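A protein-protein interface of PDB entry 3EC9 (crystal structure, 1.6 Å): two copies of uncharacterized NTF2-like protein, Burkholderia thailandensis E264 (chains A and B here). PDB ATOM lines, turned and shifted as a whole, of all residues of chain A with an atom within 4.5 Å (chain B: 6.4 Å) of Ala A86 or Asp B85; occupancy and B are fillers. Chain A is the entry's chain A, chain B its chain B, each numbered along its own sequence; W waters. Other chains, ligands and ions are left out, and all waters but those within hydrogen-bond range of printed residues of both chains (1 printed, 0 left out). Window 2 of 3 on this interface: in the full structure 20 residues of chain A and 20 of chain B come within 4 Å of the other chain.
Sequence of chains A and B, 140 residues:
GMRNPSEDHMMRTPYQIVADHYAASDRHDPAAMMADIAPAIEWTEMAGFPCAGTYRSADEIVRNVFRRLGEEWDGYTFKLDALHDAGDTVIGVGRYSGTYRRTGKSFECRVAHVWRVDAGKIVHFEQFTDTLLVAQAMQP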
ATOM      1  N   HIS A  84      29.091  13.418 -27.439  1.00  0.00           N
ATOM      2  CA  HIS A  84      28.246  12.591 -26.598  1.00  0.00           C
ATOM      3  C   HIS A  84      27.698  13.440 -25.453  1.00  0.00           C
ATOM      4  O   HIS A  84      28.477  14.063 -24.704  1.00  0.00           O
ATOM      5  CB  HIS A  84      29.039  11.414 -26.075  1.00  0.00           C
ATOM      6  CG  HIS A  84      29.683  10.575 -27.147  1.00  0.00           C
ATOM      7  ND1 HIS A  84      28.953   9.930 -28.126  1.00  0.00           N
ATOM      8  CD2 HIS A  84      30.985  10.306 -27.405  1.00  0.00           C
ATOM      9  CE1 HIS A  84      29.789   9.302 -28.936  1.00  0.00           C
ATOM     10  NE2 HIS A  84      31.031   9.503 -28.515  1.00  0.00           N
ATOM     11  N   ASP A  85      26.380  13.404 -25.253  1.00  0.00           N
ATOM     12  CA  ASP A  85      25.714  14.236 -24.309  1.00  0.00           C
ATOM     13  C   ASP A  85      25.480  13.477 -23.004  1.00  0.00           C
ATOM     14  O   ASP A  85      24.588  12.618 -22.962  1.00  0.00           O
ATOM     15  CB  ASP A  85      24.352  14.633 -24.888  1.00  0.00           C
ATOM     16  CG  ASP A  85      23.640  15.646 -24.068  1.00  0.00           C
ATOM     17  OD1 ASP A  85      24.010  15.919 -22.926  1.00  0.00           O
ATOM     18  OD2 ASP A  85      22.614  16.155 -24.592  1.00  0.00           O
ATOM     19  N   ALA A  86      26.298  13.747 -21.976  1.00  0.00           N
ATOM     20  CA  ALA A  86      26.099  13.168 -20.641  1.00  0.00           C
ATOM     21  C   ALA A  86      25.589  14.201 -19.627  1.00  0.00           C
ATOM     22  O   ALA A  86      25.944  14.175 -18.463  1.00  0.00           O
ATOM     23  CB  ALA A  86      27.341  12.418 -20.133  1.00  0.00           C
ATOM     24  N   GLY A  87      24.706  15.090 -20.066  1.00  0.00           N
ATOM     25  CA  GLY A  87      24.102  16.077 -19.179  1.00  0.00           C
ATOM     26  C   GLY A  87      25.046  17.232 -18.969  1.00  0.00           C
ATOM     27  O   GLY A  87      25.359  17.981 -19.912  1.00  0.00           O
ATOM     28  N   ASP A  88      25.545  17.362 -17.741  1.00  0.00           N
ATOM     29  CA  ASP A  88      26.522  18.413 -17.460  1.00  0.00           C
ATOM     30  C   ASP A  88      27.912  18.075 -17.974  1.00  0.00           C
ATOM     31  O   ASP A  88      28.767  18.950 -18.043  1.00  0.00           O
ATOM     32  CB  ASP A  88      26.587  18.720 -15.980  1.00  0.00           C
ATOM     33  CG  ASP A  88      25.268  19.322 -15.442  1.00  0.00           C
ATOM     34  OD1 ASP A  88      24.501  19.953 -16.213  1.00  0.00           O
ATOM     35  OD2 ASP A  88      25.000  19.138 -14.239  1.00  0.00           O
ATOM     36  N   THR A  89      28.124  16.810 -18.334  1.00  0.00           N
ATOM     37  CA  THR A  89      29.376  16.322 -18.947  1.00  0.00           C
ATOM     38  C   THR A  89      29.145  16.039 -20.392  1.00  0.00           C
ATOM     39  O   THR A  89      28.099  15.519 -20.735  1.00  0.00           O
ATOM     40  CB  THR A  89      29.946  15.089 -18.190  1.00  0.00           C
ATOM     41  OG1 THR A  89      30.125  15.477 -16.805  1.00  0.00           O
ATOM     42  CG2 THR A  89      31.248  14.555 -18.804  1.00  0.00           C
ATOM     43  N   ILE A  91      31.240  14.706 -24.044  1.00  0.00           N
ATOM     44  CA  ILE A  91      32.476  14.047 -24.501  1.00  0.00           C
ATOM     45  C   ILE A  91      32.608  14.192 -25.998  1.00  0.00           C
ATOM     46  O   ILE A  91      31.753  13.714 -26.724  1.00  0.00           O
ATOM     47  CB  ILE A  91      32.542  12.559 -24.114  1.00  0.00           C
ATOM     48  CG1 ILE A  91      32.402  12.393 -22.590  1.00  0.00           C
ATOM     49  CG2 ILE A  91      33.875  11.933 -24.610  1.00  0.00           C
ATOM     50  CD1 ILE A  91      30.995  12.440 -22.028  1.00  0.00           C
ATOM     51  N   THR B  13      20.228  -0.707 -18.283  1.00  0.00           N
ATOM     52  CA  THR B  13      20.620   0.370 -19.148  1.00  0.00           C
ATOM     53  C   THR B  13      22.023   0.090 -19.671  1.00  0.00           C
ATOM     54  O   THR B  13      22.794  -0.660 -19.069  1.00  0.00           O
ATOM     55  CB  THR B  13      20.644   1.700 -18.445  1.00  0.00           C
ATOM     56  OG1 THR B  13      21.670   1.671 -17.443  1.00  0.00           O
ATOM     57  CG2 THR B  13      19.232   2.042 -17.775  1.00  0.00           C
ATOM     58  N   PRO B  14      22.380   0.720 -20.796  1.00  0.00           N
ATOM     59  CA  PRO B  14      23.806   0.667 -21.185  1.00  0.00           C
ATOM     60  C   PRO B  14      24.819   1.011 -20.114  1.00  0.00           C
ATOM     61  O   PRO B  14      25.868   0.372 -20.004  1.00  0.00           O
ATOM     62  CB  PRO B  14      23.866   1.664 -22.365  1.00  0.00           C
ATOM     63  CG  PRO B  14      22.467   1.537 -23.017  1.00  0.00           C
ATOM     64  CD  PRO B  14      21.539   1.391 -21.815  1.00  0.00           C
ATOM     65  N   TYR B  15      24.536   2.050 -19.318  1.00  0.00           N
ATOM     66  CA  TYR B  15      25.401   2.401 -18.205  1.00  0.00           C
ATOM     67  C   TYR B  15      25.639   1.191 -17.270  1.00  0.00           C
ATOM     68  O   TYR B  15      26.760   0.893 -16.849  1.00  0.00           O
ATOM     69  CB  TYR B  15      24.777   3.586 -17.421  1.00  0.00           C
ATOM     70  CG  TYR B  15      25.519   4.038 -16.171  1.00  0.00           C
ATOM     71  CD1 TYR B  15      25.357   3.370 -14.975  1.00  0.00           C
ATOM     72  CD2 TYR B  15      26.369   5.145 -16.202  1.00  0.00           C
ATOM     73  CE1 TYR B  15      26.009   3.748 -13.827  1.00  0.00           C
ATOM     74  CE2 TYR B  15      27.032   5.550 -15.060  1.00  0.00           C
ATOM     75  CZ  TYR B  15      26.860   4.840 -13.868  1.00  0.00           C
ATOM     76  OH  TYR B  15      27.541   5.234 -12.717  1.00  0.00           O
ATOM     77  N   LEU B  83      32.119   7.549 -14.586  1.00  0.00           N
ATOM     78  CA  LEU B  83      31.381   6.818 -15.601  1.00  0.00           C
ATOM     79  C   LEU B  83      30.244   7.721 -16.057  1.00  0.00           C
ATOM     80  O   LEU B  83      29.365   8.078 -15.278  1.00  0.00           O
ATOM     81  CB  LEU B  83      30.871   5.479 -15.088  1.00  0.00           C
ATOM     82  CG  LEU B  83      30.343   4.501 -16.148  1.00  0.00           C
ATOM     83  CD1 LEU B  83      31.456   4.116 -17.131  1.00  0.00           C
ATOM     84  CD2 LEU B  83      29.735   3.266 -15.455  1.00  0.00           C
ATOM     85  N   HIS B  84      30.295   8.125 -17.327  1.00  0.00           N
ATOM     86  CA  HIS B  84      29.405   9.146 -17.834  1.00  0.00           C
ATOM     87  C   HIS B  84      28.354   8.508 -18.709  1.00  0.00           C
ATOM     88  O   HIS B  84      28.671   7.806 -19.666  1.00  0.00           O
ATOM     89  CB  HIS B  84      30.163  10.213 -18.622  1.00  0.00           C
ATOM     90  CG  HIS B  84      31.283  10.855 -17.862  1.00  0.00           C
ATOM     91  ND1 HIS B  84      31.085  11.578 -16.699  1.00  0.00           N
ATOM     92  CD2 HIS B  84      32.620  10.763 -18.033  1.00  0.00           C
ATOM     93  CE1 HIS B  84      32.272  11.962 -16.239  1.00  0.00           C
ATOM     94  NE2 HIS B  84      33.216  11.492 -17.039  1.00  0.00           N
ATOM     95  N   ASP B  85      27.096   8.755 -18.363  1.00  0.00           N
ATOM     96  CA  ASP B  85      25.947   8.146 -19.024  1.00  0.00           C
ATOM     97  C   ASP B  85      25.473   9.070 -20.140  1.00  0.00           C
ATOM     98  O   ASP B  85      24.803  10.053 -19.868  1.00  0.00           O
ATOM     99  CB  ASP B  85      24.835   7.936 -17.956  1.00  0.00           C
ATOM    100  CG  ASP B  85      23.660   7.126 -18.464  1.00  0.00           C
ATOM    101  OD1 ASP B  85      23.547   6.913 -19.672  1.00  0.00           O
ATOM    102  OD2 ASP B  85      22.802   6.703 -17.630  1.00  0.00           O
ATOM    103  N   ALA B  86      25.769   8.722 -21.404  1.00  0.00           N
ATOM    104  CA  ALA B  86      25.265   9.461 -22.578  1.00  0.00           C
ATOM    105  C   ALA B  86      24.248   8.576 -23.336  1.00  0.00           C
ATOM    106  O   ALA B  86      24.155   8.572 -24.575  1.00  0.00           O
ATOM    107  CB  ALA B  86      26.456   9.880 -23.491  1.00  0.00           C
ATOM    108  N   GLY B  87      23.494   7.779 -22.599  1.00  0.00           N
ATOM    109  CA  GLY B  87      22.379   7.038 -23.193  1.00  0.00           C
ATOM    110  C   GLY B  87      22.830   5.711 -23.762  1.00  0.00           C
ATOM    111  O   GLY B  87      23.219   4.802 -23.013  1.00  0.00           O
ATOM    112  N   ASP B  88      22.878   5.609 -25.082  1.00  0.00           N
ATOM    113  CA  ASP B  88      23.388   4.398 -25.709  1.00  0.00           C
ATOM    114  C   ASP B  88      24.897   4.349 -25.698  1.00  0.00           C
ATOM    115  O   ASP B  88      25.485   3.283 -25.899  1.00  0.00           O
ATOM    116  CB  ASP B  88      22.909   4.286 -27.143  1.00  0.00           C
ATOM    117  CG  ASP B  88      21.394   4.086 -27.238  1.00  0.00           C
ATOM    118  OD1 ASP B  88      20.808   3.552 -26.269  1.00  0.00           O
ATOM    119  OD2 ASP B  88      20.827   4.492 -28.279  1.00  0.00           O
ATOM    120  N   THR B  89      25.522   5.507 -25.497  1.00  0.00           N
ATOM    121  CA  THR B  89      26.971   5.572 -25.313  1.00  0.00           C
ATOM    122  C   THR B  89      27.259   5.795 -23.831  1.00  0.00           C
ATOM    123  O   THR B  89      26.471   6.431 -23.099  1.00  0.00           O
ATOM    124  CB  THR B  89      27.644   6.686 -26.184  1.00  0.00           C
ATOM    125  OG1 THR B  89      29.051   6.779 -25.899  1.00  0.00           O
ATOM    126  CG2 THR B  89      27.020   8.001 -25.920  1.00  0.00           C
ATOM    127  N   VAL B  90      28.382   5.240 -23.386  1.00  0.00           N
ATOM    128  CA  VAL B  90      28.789   5.357 -21.988  1.00  0.00           C
ATOM    129  C   VAL B  90      30.297   5.627 -22.042  1.00  0.00           C
ATOM    130  O   VAL B  90      30.966   5.004 -22.862  1.00  0.00           O
ATOM    131  CB  VAL B  90      28.528   4.076 -21.224  1.00  0.00           C
ATOM    132  CG1 VAL B  90      28.926   4.205 -19.711  1.00  0.00           C
ATOM    133  CG2 VAL B  90      27.050   3.663 -21.397  1.00  0.00           C
ATOM    134  N   ILE B  91      30.818   6.543 -21.214  1.00  0.00           N
ATOM    135  CA  ILE B  91      32.255   6.853 -21.239  1.00  0.00           C
ATOM    136  C   ILE B  91      32.838   6.613 -19.843  1.00  0.00           C
ATOM    137  O   ILE B  91      32.469   7.284 -18.872  1.00  0.00           O
ATOM    138  CB  ILE B  91      32.537   8.324 -21.713  1.00  0.00           C
ATOM    139  CG1 ILE B  91      31.925   8.542 -23.106  1.00  0.00           C
ATOM    140  CG2 ILE B  91      34.037   8.649 -21.709  1.00  0.00           C
ATOM    141  CD1 ILE B  91      30.423   8.916 -23.156  1.00  0.00           C
HETATM  142  O   HOH W   1      24.162  11.610 -17.647  1.00  0.00           O
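Water W1 lies within hydrogen-bond range of O of Asp B85 (2.8 Å) and O of Ala A86 (3.2 Å).
N of His A84 sits at hydrogen-bond distance from O of Ile A91 (2.8 Å). The side-chain carboxylate (OD1) of Asp A85 sits at hydrogen-bond distance from the backbone NH (N) of Gly A87. The backbone carbonyl oxygen of Ile B91 sits at hydrogen-bond distance from the backbone NH of His B84. The side-chain carboxylate of Asp B85 lies within hydrogen-bond range of the backbone NH of Gly B87, 3.1 Å away.
CB of Ala B86 touches CB of His A84, 3.96 Å away. His A84 touches Thr B89 (ND1 to CG2, 3.5 Å). O of Asp A85 touches CA of Ala B86, 3.3 Å away. CB of Ala A86 touches CB of His B84 (3.9 Å). Ala A86 touches Asp B85 (CA to O, 3.5 Å). Thr A89 touches His B84 (CG2 to ND1, 3.6 Å). Ile A91 touches Ile B91 (CD1 to CD1, 3.7 Å).
His A84 touches Ala B86, and with the chains exchanged Ala A86 touches His B84. His A84 touches Thr B89, and with the chains exchanged Thr A89 touches His B84. Asp A85 touches Ala B86, and with the chains exchanged Ala A86 touches Asp B85. Ile A91 touches its own counterpart, Ile B91. 7 positions are printed for both chains. Of the 7 pairs that touch across the chains among the printed residues, 7 have their exchanged pair printed and touching as well.
Of the printed residues of chain B, His A84 touches Ala B86 and Thr B89. Printed residues of chain B within 4 Å of Ala A86: His B84 and Asp B85. Of chain A, only Ala A86 comes within 4 Å of Asp B85. Printed residues of chain A within 4 Å of Ala B86: His A84 and Asp A85. Of the printed residues of chain A, Thr B89 touches His A84. The nearest residue of chain B that does not touch Ala A86 is Ala B86 (4.2 Å). The nearest printed residue of chain A that does not touch Thr B89 is Asp A85 (5.5 Å).
Of the 12 printed residues of chain B, 5 touch a printed residue of chain A. Hydrophobic or aromatic side chains of chain B that line the printed part of chain A: His B84, Ala B86 and Ile B91. Hydrophobic or aromatic side chains of chain A that line the printed part of chain B: His A84, Ala A86 and Ile A91. Among the printed residues, 7 pairs touch across the chains. Among the printed residues, no Asp or Glu carboxylate lies within 4 Å of a Lys or Arg side-chain nitrogen of the other chain.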
